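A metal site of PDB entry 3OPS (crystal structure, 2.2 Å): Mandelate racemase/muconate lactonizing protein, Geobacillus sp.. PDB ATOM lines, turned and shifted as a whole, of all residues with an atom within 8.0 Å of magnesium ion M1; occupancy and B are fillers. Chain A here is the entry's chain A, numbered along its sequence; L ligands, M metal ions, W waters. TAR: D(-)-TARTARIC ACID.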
ATOM      1  N   ASN A  33      -0.514  -2.093  20.695  1.00  0.00           N
ATOM      2  CA  ASN A  33       0.417  -3.157  21.007  1.00  0.00           C
ATOM      3  C   ASN A  33       0.566  -4.154  19.847  1.00  0.00           C
ATOM      4  O   ASN A  33       0.043  -3.945  18.746  1.00  0.00           O
ATOM      5  CB  ASN A  33       0.050  -3.841  22.334  1.00  0.00           C
ATOM      6  CG  ASN A  33      -1.136  -4.784  22.217  1.00  0.00           C
ATOM      7  OD1 ASN A  33      -1.620  -5.101  21.124  1.00  0.00           O
ATOM      8  ND2 ASN A  33      -1.605  -5.267  23.362  1.00  0.00           N
ATOM      9  N   TYR A 131       7.598  -1.392  37.929  1.00  0.00           N
ATOM     10  CA  TYR A 131       8.119  -1.019  36.615  1.00  0.00           C
ATOM     11  C   TYR A 131       7.142  -0.169  35.814  1.00  0.00           C
ATOM     12  O   TYR A 131       5.929  -0.264  36.006  1.00  0.00           O
ATOM     13  CB  TYR A 131       8.605  -2.236  35.814  1.00  0.00           C
ATOM     14  CG  TYR A 131       7.517  -3.178  35.327  1.00  0.00           C
ATOM     15  CD1 TYR A 131       6.779  -2.884  34.167  1.00  0.00           C
ATOM     16  CD2 TYR A 131       7.244  -4.355  35.996  1.00  0.00           C
ATOM     17  CE1 TYR A 131       5.796  -3.744  33.710  1.00  0.00           C
ATOM     18  CE2 TYR A 131       6.260  -5.215  35.556  1.00  0.00           C
ATOM     19  CZ  TYR A 131       5.537  -4.905  34.407  1.00  0.00           C
ATOM     20  OH  TYR A 131       4.554  -5.765  33.968  1.00  0.00           O
ATOM     21  N   THR A 133       5.023   0.322  32.857  1.00  0.00           N
ATOM     22  CA  THR A 133       4.435  -0.454  31.752  1.00  0.00           C
ATOM     23  C   THR A 133       3.815   0.366  30.588  1.00  0.00           C
ATOM     24  O   THR A 133       3.148  -0.199  29.719  1.00  0.00           O
ATOM     25  CB  THR A 133       3.431  -1.506  32.269  1.00  0.00           C
ATOM     26  OG1 THR A 133       3.218  -2.516  31.278  1.00  0.00           O
ATOM     27  CG2 THR A 133       2.111  -0.855  32.637  1.00  0.00           C
ATOM     28  N   TYR A 136       3.954   2.019  24.900  1.00  0.00           N
ATOM     29  CA  TYR A 136       3.198   1.366  23.841  1.00  0.00           C
ATOM     30  C   TYR A 136       3.747   1.779  22.480  1.00  0.00           C
ATOM     31  O   TYR A 136       4.648   2.610  22.423  1.00  0.00           O
ATOM     32  CB  TYR A 136       1.706   1.667  24.030  1.00  0.00           C
ATOM     33  CG  TYR A 136       1.113   0.737  25.051  1.00  0.00           C
ATOM     34  CD1 TYR A 136       1.411   0.873  26.417  1.00  0.00           C
ATOM     35  CD2 TYR A 136       0.285  -0.312  24.657  1.00  0.00           C
ATOM     36  CE1 TYR A 136       0.885  -0.012  27.358  1.00  0.00           C
ATOM     37  CE2 TYR A 136      -0.246  -1.184  25.597  1.00  0.00           C
ATOM     38  CZ  TYR A 136       0.069  -1.035  26.940  1.00  0.00           C
ATOM     39  OH  TYR A 136      -0.448  -1.935  27.848  1.00  0.00           O
ATOM     40  N   LYS A 168       9.154  -1.843  30.901  1.00  0.00           N
ATOM     41  CA  LYS A 168       8.637  -2.850  29.990  1.00  0.00           C
ATOM     42  C   LYS A 168       8.314  -2.153  28.672  1.00  0.00           C
ATOM     43  O   LYS A 168       7.470  -1.244  28.618  1.00  0.00           O
ATOM     44  CB  LYS A 168       7.405  -3.569  30.564  1.00  0.00           C
ATOM     45  CG  LYS A 168       6.947  -4.783  29.733  1.00  0.00           C
ATOM     46  CD  LYS A 168       6.246  -5.857  30.560  1.00  0.00           C
ATOM     47  CE  LYS A 168       4.746  -5.640  30.638  1.00  0.00           C
ATOM     48  NZ  LYS A 168       4.105  -6.759  31.361  1.00  0.00           N
ATOM     49  N   LYS A 170       6.999  -2.299  24.786  1.00  0.00           N
ATOM     50  CA  LYS A 170       6.133  -3.061  23.912  1.00  0.00           C
ATOM     51  C   LYS A 170       6.867  -3.305  22.623  1.00  0.00           C
ATOM     52  O   LYS A 170       7.368  -2.379  21.997  1.00  0.00           O
ATOM     53  CB  LYS A 170       4.853  -2.296  23.563  1.00  0.00           C
ATOM     54  CG  LYS A 170       3.773  -2.366  24.555  1.00  0.00           C
ATOM     55  CD  LYS A 170       3.444  -3.752  25.014  1.00  0.00           C
ATOM     56  CE  LYS A 170       2.264  -3.593  25.933  1.00  0.00           C
ATOM     57  NZ  LYS A 170       2.035  -4.710  26.879  1.00  0.00           N
ATOM     58  N   ILE A 206      10.630  -6.752  27.847  1.00  0.00           N
ATOM     59  CA  ILE A 206       9.957  -6.604  26.573  1.00  0.00           C
ATOM     60  C   ILE A 206       8.763  -7.531  26.490  1.00  0.00           C
ATOM     61  O   ILE A 206       8.778  -8.650  26.999  1.00  0.00           O
ATOM     62  CB  ILE A 206      10.931  -6.742  25.355  1.00  0.00           C
ATOM     63  CG1 ILE A 206      11.619  -8.107  25.342  1.00  0.00           C
ATOM     64  CG2 ILE A 206      11.965  -5.638  25.417  1.00  0.00           C
ATOM     65  CD1 ILE A 206      12.525  -8.352  24.133  1.00  0.00           C
ATOM     66  N   ASP A 207       7.727  -7.028  25.836  1.00  0.00           N
ATOM     67  CA  ASP A 207       6.451  -7.711  25.767  1.00  0.00           C
ATOM     68  C   ASP A 207       5.967  -7.625  24.328  1.00  0.00           C
ATOM     69  O   ASP A 207       5.679  -6.543  23.810  1.00  0.00           O
ATOM     70  CB  ASP A 207       5.495  -7.057  26.760  1.00  0.00           C
ATOM     71  CG  ASP A 207       4.077  -7.560  26.641  1.00  0.00           C
ATOM     72  OD1 ASP A 207       3.771  -8.456  25.817  1.00  0.00           O
ATOM     73  OD2 ASP A 207       3.233  -7.019  27.388  1.00  0.00           O
ATOM     74  N   ALA A 208       5.872  -8.784  23.679  1.00  0.00           N
ATOM     75  CA  ALA A 208       5.515  -8.841  22.269  1.00  0.00           C
ATOM     76  C   ALA A 208       4.018  -9.010  22.020  1.00  0.00           C
ATOM     77  O   ALA A 208       3.564  -9.000  20.872  1.00  0.00           O
ATOM     78  CB  ALA A 208       6.317  -9.901  21.565  1.00  0.00           C
ATOM     79  N   ASN A 209       3.240  -9.139  23.099  1.00  0.00           N
ATOM     80  CA  ASN A 209       1.818  -9.445  23.024  1.00  0.00           C
ATOM     81  C   ASN A 209       1.558 -10.433  21.908  1.00  0.00           C
ATOM     82  O   ASN A 209       0.749 -10.179  21.006  1.00  0.00           O
ATOM     83  CB  ASN A 209       0.972  -8.170  22.912  1.00  0.00           C
ATOM     84  CG  ASN A 209       0.905  -7.387  24.219  1.00  0.00           C
ATOM     85  OD1 ASN A 209       1.774  -6.569  24.509  1.00  0.00           O
ATOM     86  ND2 ASN A 209      -0.132  -7.657  25.018  1.00  0.00           N
ATOM     87  N   ASN A 210       2.303 -11.541  21.969  1.00  0.00           N
ATOM     88  CA  ASN A 210       2.227 -12.693  21.059  1.00  0.00           C
ATOM     89  C   ASN A 210       2.600 -12.478  19.579  1.00  0.00           C
ATOM     90  O   ASN A 210       2.513 -13.401  18.758  1.00  0.00           O
ATOM     91  CB  ASN A 210       0.904 -13.450  21.247  1.00  0.00           C
ATOM     92  CG  ASN A 210       0.754 -14.046  22.656  1.00  0.00           C
ATOM     93  OD1 ASN A 210       1.750 -14.390  23.303  1.00  0.00           O
ATOM     94  ND2 ASN A 210      -0.484 -14.204  23.123  1.00  0.00           N
ATOM     95  N   TRP A 231      13.382  -9.652  31.605  1.00  0.00           N
ATOM     96  CA  TRP A 231      12.498 -10.665  31.042  1.00  0.00           C
ATOM     97  C   TRP A 231      11.975 -10.374  29.657  1.00  0.00           C
ATOM     98  O   TRP A 231      12.175  -9.281  29.094  1.00  0.00           O
ATOM     99  CB  TRP A 231      11.400 -11.123  32.036  1.00  0.00           C
ATOM    100  CG  TRP A 231      10.127 -10.301  32.181  1.00  0.00           C
ATOM    101  CD1 TRP A 231       9.303  -9.836  31.190  1.00  0.00           C
ATOM    102  CD2 TRP A 231       9.489  -9.935  33.416  1.00  0.00           C
ATOM    103  NE1 TRP A 231       8.228  -9.185  31.724  1.00  0.00           N
ATOM    104  CE2 TRP A 231       8.306  -9.240  33.095  1.00  0.00           C
ATOM    105  CE3 TRP A 231       9.819 -10.121  34.765  1.00  0.00           C
ATOM    106  CZ2 TRP A 231       7.446  -8.710  34.067  1.00  0.00           C
ATOM    107  CZ3 TRP A 231       8.956  -9.606  35.744  1.00  0.00           C
ATOM    108  CH2 TRP A 231       7.784  -8.902  35.388  1.00  0.00           C
ATOM    109  N   GLU A 233       8.341 -11.141  27.691  1.00  0.00           N
ATOM    110  CA  GLU A 233       6.962 -11.471  27.992  1.00  0.00           C
ATOM    111  C   GLU A 233       6.139 -11.790  26.744  1.00  0.00           C
ATOM    112  O   GLU A 233       6.086 -10.984  25.813  1.00  0.00           O
ATOM    113  CB  GLU A 233       6.312 -10.336  28.770  1.00  0.00           C
ATOM    114  CG  GLU A 233       4.794 -10.421  28.861  1.00  0.00           C
ATOM    115  CD  GLU A 233       4.230  -9.424  29.833  1.00  0.00           C
ATOM    116  OE1 GLU A 233       5.054  -8.785  30.509  1.00  0.00           O
ATOM    117  OE2 GLU A 233       2.985  -9.278  29.926  1.00  0.00           O
ATOM    118  N   GLU A 234       5.513 -12.961  26.753  1.00  0.00           N
ATOM    119  CA  GLU A 234       4.645 -13.410  25.662  1.00  0.00           C
ATOM    120  C   GLU A 234       5.234 -13.106  24.282  1.00  0.00           C
ATOM    121  O   GLU A 234       4.738 -12.245  23.551  1.00  0.00           O
ATOM    122  CB  GLU A 234       3.238 -12.797  25.795  1.00  0.00           C
ATOM    123  CG  GLU A 234       2.553 -13.095  27.117  1.00  0.00           C
ATOM    124  CD  GLU A 234       1.063 -12.949  27.044  1.00  0.00           C
ATOM    125  OE1 GLU A 234       0.598 -11.869  26.603  1.00  0.00           O
ATOM    126  OE2 GLU A 234       0.333 -13.906  27.438  1.00  0.00           O
ATOM    127  N   ALA A 260       8.484 -14.728  30.868  1.00  0.00           N
ATOM    128  CA  ALA A 260       7.260 -14.376  31.574  1.00  0.00           C
ATOM    129  C   ALA A 260       6.044 -14.595  30.696  1.00  0.00           C
ATOM    130  O   ALA A 260       6.115 -14.365  29.485  1.00  0.00           O
ATOM    131  CB  ALA A 260       7.327 -12.929  32.029  1.00  0.00           C
ATOM    132  N   ASP A 261       4.945 -15.052  31.289  1.00  0.00           N
ATOM    133  CA  ASP A 261       3.724 -15.369  30.550  1.00  0.00           C
ATOM    134  C   ASP A 261       2.551 -15.599  31.524  1.00  0.00           C
ATOM    135  O   ASP A 261       2.746 -15.594  32.730  1.00  0.00           O
ATOM    136  CB  ASP A 261       3.952 -16.601  29.665  1.00  0.00           C
ATOM    137  CG  ASP A 261       3.108 -16.574  28.394  1.00  0.00           C
ATOM    138  OD1 ASP A 261       1.962 -16.056  28.428  1.00  0.00           O
ATOM    139  OD2 ASP A 261       3.578 -17.067  27.360  1.00  0.00           O
ATOM    140  N   GLY A 262       1.322 -15.774  31.013  1.00  0.00           N
ATOM    141  CA  GLY A 262       0.186 -16.024  31.921  1.00  0.00           C
ATOM    142  C   GLY A 262      -1.073 -15.173  31.811  1.00  0.00           C
ATOM    143  O   GLY A 262      -2.174 -15.698  32.020  1.00  0.00           O
ATOM    144  N   GLU A 263      -0.928 -13.886  31.509  1.00  0.00           N
ATOM    145  CA  GLU A 263      -2.077 -12.987  31.310  1.00  0.00           C
ATOM    146  C   GLU A 263      -3.009 -13.511  30.214  1.00  0.00           C
ATOM    147  O   GLU A 263      -2.671 -14.445  29.502  1.00  0.00           O
ATOM    148  CB  GLU A 263      -1.596 -11.577  30.969  1.00  0.00           C
ATOM    149  CG  GLU A 263      -1.172 -11.390  29.528  1.00  0.00           C
ATOM    150  CD  GLU A 263      -0.823  -9.946  29.183  1.00  0.00           C
ATOM    151  OE1 GLU A 263      -1.657  -9.266  28.548  1.00  0.00           O
ATOM    152  OE2 GLU A 263       0.291  -9.490  29.518  1.00  0.00           O
ATOM    153  N   GLY A 264      -4.193 -12.899  30.100  1.00  0.00           N
ATOM    154  CA  GLY A 264      -5.153 -13.246  29.043  1.00  0.00           C
ATOM    155  C   GLY A 264      -5.736 -14.628  29.254  1.00  0.00           C
ATOM    156  O   GLY A 264      -5.855 -15.095  30.396  1.00  0.00           O
ATOM    157  N   GLN A 283       2.141 -14.654  35.373  1.00  0.00           N
ATOM    158  CA  GLN A 283       1.558 -13.318  35.157  1.00  0.00           C
ATOM    159  C   GLN A 283       0.052 -13.249  35.094  1.00  0.00           C
ATOM    160  O   GLN A 283      -0.514 -12.505  34.274  1.00  0.00           O
ATOM    161  CB  GLN A 283       2.117 -12.675  33.880  1.00  0.00           C
ATOM    162  CG  GLN A 283       3.581 -12.515  33.862  1.00  0.00           C
ATOM    163  CD  GLN A 283       4.032 -11.668  32.704  1.00  0.00           C
ATOM    164  OE1 GLN A 283       3.818 -12.026  31.555  1.00  0.00           O
ATOM    165  NE2 GLN A 283       4.647 -10.536  33.004  1.00  0.00           N
ATOM    166  N   HIS A 311      -0.031  -9.560  36.488  1.00  0.00           N
ATOM    167  CA  HIS A 311      -0.466  -8.671  35.423  1.00  0.00           C
ATOM    168  C   HIS A 311      -1.383  -7.636  35.988  1.00  0.00           C
ATOM    169  O   HIS A 311      -2.200  -7.916  36.895  1.00  0.00           O
ATOM    170  CB  HIS A 311      -1.226  -9.453  34.326  1.00  0.00           C
ATOM    171  CG  HIS A 311      -1.827  -8.592  33.264  1.00  0.00           C
ATOM    172  ND1 HIS A 311      -2.999  -7.887  33.435  1.00  0.00           N
ATOM    173  CD2 HIS A 311      -1.428  -8.331  31.990  1.00  0.00           C
ATOM    174  CE1 HIS A 311      -3.298  -7.221  32.335  1.00  0.00           C
ATOM    175  NE2 HIS A 311      -2.358  -7.484  31.437  1.00  0.00           N
ATOM    176  N   CYS A 312      -1.273  -6.434  35.447  1.00  0.00           N
ATOM    177  CA  CYS A 312      -2.191  -5.367  35.772  1.00  0.00           C
ATOM    178  C   CYS A 312      -2.138  -4.309  34.709  1.00  0.00           C
ATOM    179  O   CYS A 312      -1.085  -3.733  34.441  1.00  0.00           O
ATOM    180  CB  CYS A 312      -1.879  -4.753  37.125  1.00  0.00           C
ATOM    181  SG  CYS A 312      -3.126  -3.576  37.626  1.00  0.00           S
ATOM    182  N   TYR A 313      -3.290  -4.071  34.095  1.00  0.00           N
ATOM    183  CA  TYR A 313      -3.457  -3.035  33.089  1.00  0.00           C
ATOM    184  C   TYR A 313      -4.929  -2.942  32.777  1.00  0.00           C
ATOM    185  O   TYR A 313      -5.603  -3.961  32.564  1.00  0.00           O
ATOM    186  CB  TYR A 313      -2.677  -3.365  31.820  1.00  0.00           C
ATOM    187  CG  TYR A 313      -2.507  -2.152  30.934  1.00  0.00           C
ATOM    188  CD1 TYR A 313      -1.489  -1.233  31.180  1.00  0.00           C
ATOM    189  CD2 TYR A 313      -3.372  -1.921  29.868  1.00  0.00           C
ATOM    190  CE1 TYR A 313      -1.335  -0.121  30.381  1.00  0.00           C
ATOM    191  CE2 TYR A 313      -3.217  -0.808  29.069  1.00  0.00           C
ATOM    192  CZ  TYR A 313      -2.210   0.091  29.327  1.00  0.00           C
ATOM    193  OH  TYR A 313      -2.049   1.208  28.540  1.00  0.00           O
ATOM    194  N   GLU A 336       3.468  -3.884  38.253  1.00  0.00           N
ATOM    195  CA  GLU A 336       3.225  -3.324  36.920  1.00  0.00           C
ATOM    196  C   GLU A 336       2.538  -1.958  37.025  1.00  0.00           C
ATOM    197  O   GLU A 336       1.310  -1.879  37.072  1.00  0.00           O
ATOM    198  CB  GLU A 336       2.392  -4.292  36.091  1.00  0.00           C
ATOM    199  CG  GLU A 336       2.044  -3.744  34.712  1.00  0.00           C
ATOM    200  CD  GLU A 336       1.677  -4.818  33.687  1.00  0.00           C
ATOM    201  OE1 GLU A 336       1.330  -5.957  34.053  1.00  0.00           O
ATOM    202  OE2 GLU A 336       1.742  -4.496  32.499  1.00  0.00           O
HETATM  203  O1  TAR L   1       0.287  -4.682  30.281  1.00  0.00           O
HETATM  204  O11 TAR L   1       1.297  -6.614  30.239  1.00  0.00           O
HETATM  205  C1  TAR L   1       0.416  -5.826  29.814  1.00  0.00           C
HETATM  206  C2  TAR L   1      -0.531  -6.279  28.718  1.00  0.00           C
HETATM  207  O2  TAR L   1       0.188  -6.728  27.551  1.00  0.00           O
HETATM  208  C3  TAR L   1      -1.551  -5.187  28.386  1.00  0.00           C
HETATM  209  O3  TAR L   1      -2.774  -5.597  28.992  1.00  0.00           O
HETATM  210  C4  TAR L   1      -1.730  -4.939  26.904  1.00  0.00           C
HETATM  211  O4  TAR L   1      -0.947  -4.120  26.365  1.00  0.00           O
HETATM  212  O41 TAR L   1      -2.631  -5.547  26.261  1.00  0.00           O
HETATM  213 MG    MG M   1       1.623  -8.536  28.558  1.00  0.00          MG
HETATM  214 MG    MG M   2       0.603 -16.026  26.898  1.00  0.00          MG
HETATM  215  O   HOH W   1       1.471  -9.735  26.917  1.00  0.00           O
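The side-chain carboxylate (OE1) of Glu 263 is in hydrogen-bond range of a ring nitrogen (NE2) of His 311 (3.5 Å).
The side-chain amino group (NZ) of Lys 168 lies close to the side-chain carboxylate (OE2) of Glu 233 (3.1 Å).
The side-chain amide nitrogen (NE2) of Gln 283 is in hydrogen-bond range of the side-chain carboxylate (OE1) of Glu 233, at 3.1 Å.
O of Ile 206 lies within hydrogen-bond range of N of Glu 233 (2.6 Å).
The indole nitrogen (NE1) of Trp 231 sits at hydrogen-bond distance from the side-chain carboxylate (OE1) of Glu 233 (3.4 Å).
The backbone carbonyl oxygen (O) of Glu 234 lies within hydrogen-bond range of the backbone NH (N) of Asn 209 (3.5 Å).
O of Glu 234 sits at hydrogen-bond distance from N of Asn 210 (3.0 Å).
The backbone NH (N) of Glu 234 sits at hydrogen-bond distance from the backbone carbonyl oxygen (O) of Ala 260 (3.1 Å).
Water W1 bridges OD1 of Asp 207 (2.9 Å) and ND2 of Asn 209 (3.2 Å).
Residues that only touch magnesium ion M1: Glu 234.
Magnesium ion M1 is bound by OE2 of Glu 263 (1.9 Å), water W1 (2.0 Å), OE2 of Glu 233 (2.1 Å), OD2 of Asp 207 (2.5 Å), O2 of the ligand (2.5 Å) and O11 of the ligand (2.6 Å).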
